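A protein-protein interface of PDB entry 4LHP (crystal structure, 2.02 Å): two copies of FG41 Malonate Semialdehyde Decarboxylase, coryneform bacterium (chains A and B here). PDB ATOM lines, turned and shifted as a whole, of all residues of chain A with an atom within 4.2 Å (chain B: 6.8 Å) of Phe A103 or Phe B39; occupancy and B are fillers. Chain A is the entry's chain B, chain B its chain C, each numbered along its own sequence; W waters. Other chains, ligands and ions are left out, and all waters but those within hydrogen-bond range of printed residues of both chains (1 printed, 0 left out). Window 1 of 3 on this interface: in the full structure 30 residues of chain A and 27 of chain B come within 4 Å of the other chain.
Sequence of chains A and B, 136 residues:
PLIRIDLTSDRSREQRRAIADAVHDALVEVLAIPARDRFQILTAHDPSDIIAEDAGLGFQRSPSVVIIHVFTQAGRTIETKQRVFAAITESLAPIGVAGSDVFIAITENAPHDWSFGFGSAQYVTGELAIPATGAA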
ATOM      1  N   ILE A  51       3.855 -24.491 -11.097  1.00  0.00           N
ATOM      2  CA  ILE A  51       4.287 -23.514 -12.079  1.00  0.00           C
ATOM      3  C   ILE A  51       3.144 -22.555 -12.374  1.00  0.00           C
ATOM      4  O   ILE A  51       2.160 -22.923 -13.011  1.00  0.00           O
ATOM      5  CB  ILE A  51       4.726 -24.213 -13.371  1.00  0.00           C
ATOM      6  CG1 ILE A  51       5.804 -25.251 -13.046  1.00  0.00           C
ATOM      7  CG2 ILE A  51       5.224 -23.197 -14.385  1.00  0.00           C
ATOM      8  CD1 ILE A  51       6.305 -26.037 -14.237  1.00  0.00           C
ATOM      9  N   ALA A  52       3.277 -21.326 -11.890  1.00  0.00           N
ATOM     10  CA  ALA A  52       2.249 -20.310 -12.074  1.00  0.00           C
ATOM     11  C   ALA A  52       2.894 -18.973 -12.401  1.00  0.00           C
ATOM     12  O   ALA A  52       3.514 -18.345 -11.542  1.00  0.00           O
ATOM     13  CB  ALA A  52       1.396 -20.191 -10.823  1.00  0.00           C
ATOM     14  N   GLU A  53       2.749 -18.547 -13.651  1.00  0.00           N
ATOM     15  CA  GLU A  53       3.292 -17.271 -14.092  1.00  0.00           C
ATOM     16  C   GLU A  53       2.193 -16.208 -13.978  1.00  0.00           C
ATOM     17  O   GLU A  53       1.438 -16.228 -13.007  1.00  0.00           O
ATOM     18  CB  GLU A  53       3.881 -17.418 -15.499  1.00  0.00           C
ATOM     19  CG  GLU A  53       4.943 -18.528 -15.546  1.00  0.00           C
ATOM     20  CD  GLU A  53       5.697 -18.613 -16.862  1.00  0.00           C
ATOM     21  OE1 GLU A  53       5.214 -18.065 -17.871  1.00  0.00           O
ATOM     22  OE2 GLU A  53       6.781 -19.235 -16.884  1.00  0.00           O
ATOM     23  N   ARG A  61       5.567 -13.679  -8.928  1.00  0.00           N
ATOM     24  CA  ARG A  61       5.165 -14.394  -7.733  1.00  0.00           C
ATOM     25  C   ARG A  61       6.411 -14.902  -7.029  1.00  0.00           C
ATOM     26  O   ARG A  61       7.478 -14.995  -7.637  1.00  0.00           O
ATOM     27  CB  ARG A  61       4.278 -15.577  -8.118  1.00  0.00           C
ATOM     28  CG  ARG A  61       3.425 -15.319  -9.347  1.00  0.00           C
ATOM     29  CD  ARG A  61       2.481 -16.472  -9.634  1.00  0.00           C
ATOM     30  NE  ARG A  61       1.203 -16.314  -8.947  1.00  0.00           N
ATOM     31  CZ  ARG A  61       0.047 -16.018  -9.539  1.00  0.00           C
ATOM     32  NH1 ARG A  61      -0.034 -15.854 -10.852  1.00  0.00           N
ATOM     33  NH2 ARG A  61      -1.047 -15.893  -8.804  1.00  0.00           N
ATOM     34  N   VAL A  66       0.154 -20.581  -3.945  1.00  0.00           N
ATOM     35  CA  VAL A  66      -0.947 -21.387  -3.439  1.00  0.00           C
ATOM     36  C   VAL A  66      -2.075 -21.416  -4.465  1.00  0.00           C
ATOM     37  O   VAL A  66      -2.713 -20.398  -4.737  1.00  0.00           O
ATOM     38  CB  VAL A  66      -1.480 -20.833  -2.110  1.00  0.00           C
ATOM     39  CG1 VAL A  66      -2.674 -21.646  -1.633  1.00  0.00           C
ATOM     40  CG2 VAL A  66      -0.376 -20.830  -1.060  1.00  0.00           C
ATOM     41  N   ILE A  67      -2.305 -22.587  -5.045  1.00  0.00           N
ATOM     42  CA  ILE A  67      -3.379 -22.766  -6.011  1.00  0.00           C
ATOM     43  C   ILE A  67      -4.597 -23.360  -5.313  1.00  0.00           C
ATOM     44  O   ILE A  67      -4.505 -24.401  -4.667  1.00  0.00           O
ATOM     45  CB  ILE A  67      -2.945 -23.692  -7.155  1.00  0.00           C
ATOM     46  CG1 ILE A  67      -1.773 -23.067  -7.912  1.00  0.00           C
ATOM     47  CG2 ILE A  67      -4.114 -23.953  -8.093  1.00  0.00           C
ATOM     48  CD1 ILE A  67      -1.205 -23.942  -9.008  1.00  0.00           C
ATOM     49  N   ILE A  68      -5.735 -22.687  -5.445  1.00  0.00           N
ATOM     50  CA  ILE A  68      -6.965 -23.123  -4.802  1.00  0.00           C
ATOM     51  C   ILE A  68      -8.020 -23.431  -5.860  1.00  0.00           C
ATOM     52  O   ILE A  68      -8.403 -22.559  -6.637  1.00  0.00           O
ATOM     53  CB  ILE A  68      -7.493 -22.044  -3.841  1.00  0.00           C
ATOM     54  CG1 ILE A  68      -6.428 -21.704  -2.792  1.00  0.00           C
ATOM     55  CG2 ILE A  68      -8.765 -22.517  -3.158  1.00  0.00           C
ATOM     56  CD1 ILE A  68      -6.512 -20.293  -2.265  1.00  0.00           C
ATOM     57  N   ASP A 101       0.598 -14.460  -4.919  1.00  0.00           N
ATOM     58  CA  ASP A 101       0.895 -15.886  -4.878  1.00  0.00           C
ATOM     59  C   ASP A 101      -0.354 -16.762  -4.865  1.00  0.00           C
ATOM     60  O   ASP A 101      -0.253 -17.983  -4.748  1.00  0.00           O
ATOM     61  CB  ASP A 101       1.752 -16.198  -3.650  1.00  0.00           C
ATOM     62  CG  ASP A 101       3.131 -15.576  -3.728  1.00  0.00           C
ATOM     63  OD1 ASP A 101       3.524 -15.122  -4.824  1.00  0.00           O
ATOM     64  OD2 ASP A 101       3.830 -15.552  -2.694  1.00  0.00           O
ATOM     65  N   VAL A 102      -1.526 -16.148  -4.983  1.00  0.00           N
ATOM     66  CA  VAL A 102      -2.775 -16.899  -4.964  1.00  0.00           C
ATOM     67  C   VAL A 102      -3.338 -17.064  -6.368  1.00  0.00           C
ATOM     68  O   VAL A 102      -3.409 -16.107  -7.134  1.00  0.00           O
ATOM     69  CB  VAL A 102      -3.840 -16.213  -4.083  1.00  0.00           C
ATOM     70  CG1 VAL A 102      -5.150 -16.995  -4.116  1.00  0.00           C
ATOM     71  CG2 VAL A 102      -3.334 -16.060  -2.658  1.00  0.00           C
ATOM     72  N   PHE A 103      -3.727 -18.290  -6.697  1.00  0.00           N
ATOM     73  CA  PHE A 103      -4.398 -18.581  -7.956  1.00  0.00           C
ATOM     74  C   PHE A 103      -5.665 -19.365  -7.633  1.00  0.00           C
ATOM     75  O   PHE A 103      -5.614 -20.360  -6.909  1.00  0.00           O
ATOM     76  CB  PHE A 103      -3.480 -19.395  -8.871  1.00  0.00           C
ATOM     77  CG  PHE A 103      -4.066 -19.683 -10.227  1.00  0.00           C
ATOM     78  CD1 PHE A 103      -3.741 -18.896 -11.317  1.00  0.00           C
ATOM     79  CD2 PHE A 103      -4.934 -20.746 -10.411  1.00  0.00           C
ATOM     80  CE1 PHE A 103      -4.273 -19.159 -12.566  1.00  0.00           C
ATOM     81  CE2 PHE A 103      -5.471 -21.015 -11.657  1.00  0.00           C
ATOM     82  CZ  PHE A 103      -5.141 -20.219 -12.736  1.00  0.00           C
ATOM     83  N   ILE A 104      -6.802 -18.914  -8.151  1.00  0.00           N
ATOM     84  CA  ILE A 104      -8.070 -19.567  -7.860  1.00  0.00           C
ATOM     85  C   ILE A 104      -8.791 -19.944  -9.144  1.00  0.00           C
ATOM     86  O   ILE A 104      -8.844 -19.158 -10.091  1.00  0.00           O
ATOM     87  CB  ILE A 104      -9.007 -18.667  -7.032  1.00  0.00           C
ATOM     88  CG1 ILE A 104      -8.252 -18.023  -5.867  1.00  0.00           C
ATOM     89  CG2 ILE A 104     -10.187 -19.474  -6.521  1.00  0.00           C
ATOM     90  CD1 ILE A 104      -9.039 -16.931  -5.162  1.00  0.00           C
ATOM     91  N   PRO B   1      -5.444 -21.659 -18.840  1.00  0.00           N
ATOM     92  CA  PRO B   1      -5.871 -22.960 -18.311  1.00  0.00           C
ATOM     93  C   PRO B   1      -5.040 -23.409 -17.115  1.00  0.00           C
ATOM     94  O   PRO B   1      -3.912 -22.944 -16.948  1.00  0.00           O
ATOM     95  CB  PRO B   1      -5.627 -23.907 -19.488  1.00  0.00           C
ATOM     96  CG  PRO B   1      -4.474 -23.298 -20.216  1.00  0.00           C
ATOM     97  CD  PRO B   1      -4.542 -21.805 -19.997  1.00  0.00           C
ATOM     98  N   LEU B   2      -5.601 -24.300 -16.300  1.00  0.00           N
ATOM     99  CA  LEU B   2      -4.876 -24.919 -15.198  1.00  0.00           C
ATOM    100  C   LEU B   2      -4.694 -26.396 -15.512  1.00  0.00           C
ATOM    101  O   LEU B   2      -5.670 -27.116 -15.710  1.00  0.00           O
ATOM    102  CB  LEU B   2      -5.651 -24.764 -13.891  1.00  0.00           C
ATOM    103  CG  LEU B   2      -5.055 -25.492 -12.682  1.00  0.00           C
ATOM    104  CD1 LEU B   2      -3.736 -24.865 -12.268  1.00  0.00           C
ATOM    105  CD2 LEU B   2      -6.037 -25.503 -11.519  1.00  0.00           C
ATOM    106  N   ILE B   3      -3.448 -26.850 -15.554  1.00  0.00           N
ATOM    107  CA  ILE B   3      -3.165 -28.220 -15.966  1.00  0.00           C
ATOM    108  C   ILE B   3      -2.627 -29.058 -14.819  1.00  0.00           C
ATOM    109  O   ILE B   3      -1.575 -28.754 -14.259  1.00  0.00           O
ATOM    110  CB  ILE B   3      -2.132 -28.264 -17.105  1.00  0.00           C
ATOM    111  CG1 ILE B   3      -2.360 -27.112 -18.087  1.00  0.00           C
ATOM    112  CG2 ILE B   3      -2.195 -29.604 -17.812  1.00  0.00           C
ATOM    113  CD1 ILE B   3      -3.718 -27.118 -18.733  1.00  0.00           C
ATOM    114  N   ARG B   4      -3.351 -30.115 -14.473  1.00  0.00           N
ATOM    115  CA  ARG B   4      -2.853 -31.088 -13.512  1.00  0.00           C
ATOM    116  C   ARG B   4      -2.165 -32.225 -14.251  1.00  0.00           C
ATOM    117  O   ARG B   4      -2.778 -32.917 -15.063  1.00  0.00           O
ATOM    118  CB  ARG B   4      -3.984 -31.607 -12.625  1.00  0.00           C
ATOM    119  CG  ARG B   4      -4.478 -30.542 -11.680  1.00  0.00           C
ATOM    120  CD  ARG B   4      -5.654 -30.957 -10.830  1.00  0.00           C
ATOM    121  NE  ARG B   4      -6.143 -29.782 -10.115  1.00  0.00           N
ATOM    122  CZ  ARG B   4      -5.788 -29.440  -8.879  1.00  0.00           C
ATOM    123  NH1 ARG B   4      -4.964 -30.197  -8.170  1.00  0.00           N
ATOM    124  NH2 ARG B   4      -6.272 -28.336  -8.333  1.00  0.00           N
ATOM    125  N   HIS B  24       2.914 -27.272 -22.224  1.00  0.00           N
ATOM    126  CA  HIS B  24       2.643 -25.848 -22.358  1.00  0.00           C
ATOM    127  C   HIS B  24       2.931 -25.333 -23.766  1.00  0.00           C
ATOM    128  O   HIS B  24       2.150 -24.555 -24.309  1.00  0.00           O
ATOM    129  CB  HIS B  24       3.433 -25.033 -21.339  1.00  0.00           C
ATOM    130  CG  HIS B  24       3.152 -23.566 -21.413  1.00  0.00           C
ATOM    131  ND1 HIS B  24       1.944 -23.025 -21.030  1.00  0.00           N
ATOM    132  CD2 HIS B  24       3.907 -22.533 -21.853  1.00  0.00           C
ATOM    133  CE1 HIS B  24       1.971 -21.719 -21.218  1.00  0.00           C
ATOM    134  NE2 HIS B  24       3.150 -21.393 -21.716  1.00  0.00           N
ATOM    135  N   ARG B  36       2.763 -16.621 -21.287  1.00  0.00           N
ATOM    136  CA  ARG B  36       2.914 -16.681 -19.839  1.00  0.00           C
ATOM    137  C   ARG B  36       1.640 -17.141 -19.133  1.00  0.00           C
ATOM    138  O   ARG B  36       1.567 -17.129 -17.905  1.00  0.00           O
ATOM    139  CB  ARG B  36       3.350 -15.321 -19.297  1.00  0.00           C
ATOM    140  CG  ARG B  36       4.721 -14.880 -19.781  1.00  0.00           C
ATOM    141  CD  ARG B  36       5.232 -13.709 -18.965  1.00  0.00           C
ATOM    142  NE  ARG B  36       5.336 -14.053 -17.551  1.00  0.00           N
ATOM    143  CZ  ARG B  36       6.383 -14.653 -16.992  1.00  0.00           C
ATOM    144  NH1 ARG B  36       7.441 -14.985 -17.722  1.00  0.00           N
ATOM    145  NH2 ARG B  36       6.370 -14.928 -15.696  1.00  0.00           N
ATOM    146  N   ASP B  37       0.642 -17.555 -19.908  1.00  0.00           N
ATOM    147  CA  ASP B  37      -0.572 -18.125 -19.338  1.00  0.00           C
ATOM    148  C   ASP B  37      -0.279 -19.568 -18.954  1.00  0.00           C
ATOM    149  O   ASP B  37      -0.921 -20.500 -19.441  1.00  0.00           O
ATOM    150  CB  ASP B  37      -1.725 -18.066 -20.341  1.00  0.00           C
ATOM    151  CG  ASP B  37      -3.073 -18.329 -19.695  1.00  0.00           C
ATOM    152  OD1 ASP B  37      -3.100 -18.723 -18.510  1.00  0.00           O
ATOM    153  OD2 ASP B  37      -4.105 -18.145 -20.373  1.00  0.00           O
ATOM    154  N   ARG B  38       0.703 -19.740 -18.076  1.00  0.00           N
ATOM    155  CA  ARG B  38       1.200 -21.060 -17.719  1.00  0.00           C
ATOM    156  C   ARG B  38       0.880 -21.386 -16.266  1.00  0.00           C
ATOM    157  O   ARG B  38       1.387 -20.745 -15.343  1.00  0.00           O
ATOM    158  CB  ARG B  38       2.708 -21.133 -17.951  1.00  0.00           C
ATOM    159  CG  ARG B  38       3.331 -22.416 -17.448  1.00  0.00           C
ATOM    160  CD  ARG B  38       4.746 -22.615 -17.952  1.00  0.00           C
ATOM    161  NE  ARG B  38       5.176 -23.981 -17.684  1.00  0.00           N
ATOM    162  CZ  ARG B  38       6.243 -24.566 -18.213  1.00  0.00           C
ATOM    163  NH1 ARG B  38       7.024 -23.913 -19.065  1.00  0.00           N
ATOM    164  NH2 ARG B  38       6.519 -25.819 -17.888  1.00  0.00           N
ATOM    165  N   PHE B  39       0.035 -22.391 -16.070  1.00  0.00           N
ATOM    166  CA  PHE B  39      -0.389 -22.780 -14.735  1.00  0.00           C
ATOM    167  C   PHE B  39      -0.516 -24.290 -14.643  1.00  0.00           C
ATOM    168  O   PHE B  39      -1.443 -24.885 -15.188  1.00  0.00           O
ATOM    169  CB  PHE B  39      -1.702 -22.089 -14.380  1.00  0.00           C
ATOM    170  CG  PHE B  39      -1.607 -20.592 -14.413  1.00  0.00           C
ATOM    171  CD1 PHE B  39      -2.062 -19.876 -15.506  1.00  0.00           C
ATOM    172  CD2 PHE B  39      -1.026 -19.904 -13.362  1.00  0.00           C
ATOM    173  CE1 PHE B  39      -1.959 -18.498 -15.538  1.00  0.00           C
ATOM    174  CE2 PHE B  39      -0.919 -18.529 -13.389  1.00  0.00           C
ATOM    175  CZ  PHE B  39      -1.384 -17.826 -14.478  1.00  0.00           C
ATOM    176  N   GLN B  40       0.434 -24.902 -13.947  1.00  0.00           N
ATOM    177  CA  GLN B  40       0.566 -26.348 -13.950  1.00  0.00           C
ATOM    178  C   GLN B  40       0.893 -26.864 -12.560  1.00  0.00           C
ATOM    179  O   GLN B  40       1.631 -26.229 -11.806  1.00  0.00           O
ATOM    180  CB  GLN B  40       1.678 -26.761 -14.916  1.00  0.00           C
ATOM    181  CG  GLN B  40       1.558 -26.150 -16.302  1.00  0.00           C
ATOM    182  CD  GLN B  40       2.772 -26.441 -17.165  1.00  0.00           C
ATOM    183  OE1 GLN B  40       3.908 -26.380 -16.695  1.00  0.00           O
ATOM    184  NE2 GLN B  40       2.538 -26.768 -18.430  1.00  0.00           N
ATOM    185  N   ILE B  41       0.331 -28.020 -12.228  1.00  0.00           N
ATOM    186  CA  ILE B  41       0.650 -28.704 -10.987  1.00  0.00           C
ATOM    187  C   ILE B  41       1.157 -30.105 -11.297  1.00  0.00           C
ATOM    188  O   ILE B  41       0.399 -30.969 -11.742  1.00  0.00           O
ATOM    189  CB  ILE B  41      -0.572 -28.795 -10.067  1.00  0.00           C
ATOM    190  CG1 ILE B  41      -1.072 -27.392  -9.723  1.00  0.00           C
ATOM    191  CG2 ILE B  41      -0.224 -29.560  -8.799  1.00  0.00           C
ATOM    192  CD1 ILE B  41      -2.439 -27.371  -9.080  1.00  0.00           C
ATOM    193  N   TRP B 114     -12.203 -17.605 -12.734  1.00  0.00           N
ATOM    194  CA  TRP B 114     -10.750 -17.522 -12.611  1.00  0.00           C
ATOM    195  C   TRP B 114     -10.278 -16.281 -11.860  1.00  0.00           C
ATOM    196  O   TRP B 114     -10.728 -15.169 -12.132  1.00  0.00           O
ATOM    197  CB  TRP B 114     -10.107 -17.513 -13.999  1.00  0.00           C
ATOM    198  CG  TRP B 114     -10.336 -18.756 -14.795  1.00  0.00           C
ATOM    199  CD1 TRP B 114     -11.322 -18.971 -15.711  1.00  0.00           C
ATOM    200  CD2 TRP B 114      -9.558 -19.957 -14.753  1.00  0.00           C
ATOM    201  NE1 TRP B 114     -11.209 -20.232 -16.243  1.00  0.00           N
ATOM    202  CE2 TRP B 114     -10.133 -20.859 -15.671  1.00  0.00           C
ATOM    203  CE3 TRP B 114      -8.432 -20.359 -14.029  1.00  0.00           C
ATOM    204  CZ2 TRP B 114      -9.620 -22.137 -15.883  1.00  0.00           C
ATOM    205  CZ3 TRP B 114      -7.925 -21.630 -14.240  1.00  0.00           C
ATOM    206  CH2 TRP B 114      -8.520 -22.503 -15.161  1.00  0.00           C
ATOM    207  N   SER B 115      -9.362 -16.484 -10.918  1.00  0.00           N
ATOM    208  CA  SER B 115      -8.602 -15.388 -10.329  1.00  0.00           C
ATOM    209  C   SER B 115      -7.111 -15.685 -10.457  1.00  0.00           C
ATOM    210  O   SER B 115      -6.627 -16.688  -9.939  1.00  0.00           O
ATOM    211  CB  SER B 115      -8.981 -15.191  -8.862  1.00  0.00           C
ATOM    212  OG  SER B 115      -8.213 -14.155  -8.269  1.00  0.00           O
ATOM    213  N   PHE B 116      -6.392 -14.811 -11.157  1.00  0.00           N
ATOM    214  CA  PHE B 116      -4.969 -15.013 -11.414  1.00  0.00           C
ATOM    215  C   PHE B 116      -4.094 -14.441 -10.311  1.00  0.00           C
ATOM    216  O   PHE B 116      -2.884 -14.649 -10.306  1.00  0.00           O
ATOM    217  CB  PHE B 116      -4.576 -14.363 -12.743  1.00  0.00           C
ATOM    218  CG  PHE B 116      -5.177 -15.031 -13.946  1.00  0.00           C
ATOM    219  CD1 PHE B 116      -4.457 -15.972 -14.662  1.00  0.00           C
ATOM    220  CD2 PHE B 116      -6.463 -14.720 -14.360  1.00  0.00           C
ATOM    221  CE1 PHE B 116      -5.005 -16.589 -15.770  1.00  0.00           C
ATOM    222  CE2 PHE B 116      -7.016 -15.336 -15.467  1.00  0.00           C
ATOM    223  CZ  PHE B 116      -6.286 -16.271 -16.172  1.00  0.00           C
ATOM    224  N   GLY B 117      -4.703 -13.708  -9.387  1.00  0.00           N
ATOM    225  CA  GLY B 117      -3.974 -13.127  -8.278  1.00  0.00           C
ATOM    226  C   GLY B 117      -4.683 -11.917  -7.709  1.00  0.00           C
ATOM    227  O   GLY B 117      -5.561 -11.335  -8.352  1.00  0.00           O
ATOM    228  N   PHE B 118      -4.316 -11.562  -6.484  1.00  0.00           N
ATOM    229  CA  PHE B 118      -4.758 -10.319  -5.865  1.00  0.00           C
ATOM    230  C   PHE B 118      -6.262 -10.285  -5.593  1.00  0.00           C
ATOM    231  O   PHE B 118      -6.835  -9.218  -5.379  1.00  0.00           O
ATOM    232  CB  PHE B 118      -4.350  -9.129  -6.738  1.00  0.00           C
ATOM    233  CG  PHE B 118      -2.894  -9.127  -7.106  1.00  0.00           C
ATOM    234  CD1 PHE B 118      -2.490  -9.462  -8.387  1.00  0.00           C
ATOM    235  CD2 PHE B 118      -1.927  -8.811  -6.164  1.00  0.00           C
ATOM    236  CE1 PHE B 118      -1.150  -9.469  -8.728  1.00  0.00           C
ATOM    237  CE2 PHE B 118      -0.586  -8.819  -6.496  1.00  0.00           C
ATOM    238  CZ  PHE B 118      -0.197  -9.147  -7.780  1.00  0.00           C
HETATM  239  O   HOH W   1      -5.259 -26.952  -6.440  1.00  0.00           O
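The backbone NH of Ile A68 is in hydrogen-bond range of the backbone carbonyl oxygen of Phe A103 (2.8 Å).
The side-chain amide oxygen of Gln B40 lies within hydrogen-bond range of the guanidinium group of Arg B38.
The backbone carbonyl oxygen of Phe B39 sits at hydrogen-bond distance from the backbone NH of Ile B3.
O of Val A102 sits at hydrogen-bond distance from NH2 of Arg A61 (2.9 Å).
NH1 of Arg A61 lies within hydrogen-bond range of O of Glu A53 (2.6 Å).
N of Phe A103 is in hydrogen-bond range of O of Val A66.
Of the 16 printed residues of chain B, 9 touch a printed residue of chain A.
Printed residues of chain A that touch a printed residue of chain B: Ile A51, Ala A52, Glu A53, Arg A61, Ile A67, Val A102, Phe A103 and Ile A104.
Among the printed residues, 19 pairs touch across the chains.
The guanidinium group of Arg A61 lies within hydrogen-bond range of the backbone carbonyl oxygen of Phe B116 (2.7 Å).
NH1 of Arg B36 lies within salt-bridge range of OE1 of Glu A53 (3.8 Å).
The backbone NH of Ser B115 is in hydrogen-bond range of the backbone carbonyl oxygen of Ile A104, 2.8 Å away.
The backbone NH (N) of Gln B40 lies within hydrogen-bond range of the backbone carbonyl oxygen (O) of Ile A51, 2.8 Å away.
The backbone carbonyl oxygen (O) of Arg B38 is in hydrogen-bond range of the backbone NH (N) of Glu A53, at 3.1 Å.
The backbone carbonyl oxygen (O) of Ile A51 sits close to the backbone carbonyl oxygen (O) of Arg B38 (3.3 Å).
No position is printed for both chains.
Of the 19 pairs that touch across the chains among the printed residues, none has its exchanged pair printed and touching as well.
Water W1 lies within hydrogen-bond range of the guanidinium group of Arg B4 (2.6 Å) and the backbone carbonyl oxygen of Ile A67 (3.2 Å).
Phe B39 touches Ile A51 (CA to O, 3.1 Å).
Phe B39 touches Ala A52 (CD2 to CB, 3.5 Å).
Glu A53 touches Phe B39 (O to CE2, 3.3 Å).
Phe B39 touches Arg A61.
Ile B41 touches Ile A67.
Val A102 touches Phe B116 (O to O, 3.5 Å).
Gly B117 touches Val A102 (CA to O, 3.2 Å).
CZ of Phe A103 touches CZ3 of Trp B114, 3.5 Å away.
CA of Phe A103 touches O of Ser B115, at 3.5 Å.
Phe B116 touches Phe A103 (CD1 to CE1, 3.8 Å).
Of the printed residues of chain B, Phe A103 touches Phe B39 (3.4 Å), Trp B114 (3.5 Å), Ser B115 (3.5 Å) and Phe B116 (3.8 Å).
Phe B39 touches just these residues of chain A: Ile A51, Ala A52, Glu A53, Arg A61 and Phe A103.
Of the printed residues of chain B, Glu A53 touches Arg B36 (3.3 Å), Arg B38 (3.1 Å) and Phe B39 (3.3 Å).
Printed residues of chain A within 4 Å of Gln B40: Ile A51 (2.8 Å).
Printed residues of chain B within 4 Å of Ile A67: Ile B41 (3.5 Å).
Printed residues of chain A within 4 Å of Trp B114: Phe A103 and Ile A104.
Leu B2 touches none of the printed residues of chain A.
The nearest printed residue of chain A that does not touch Phe B39 is Ile A67 (5.7 Å).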
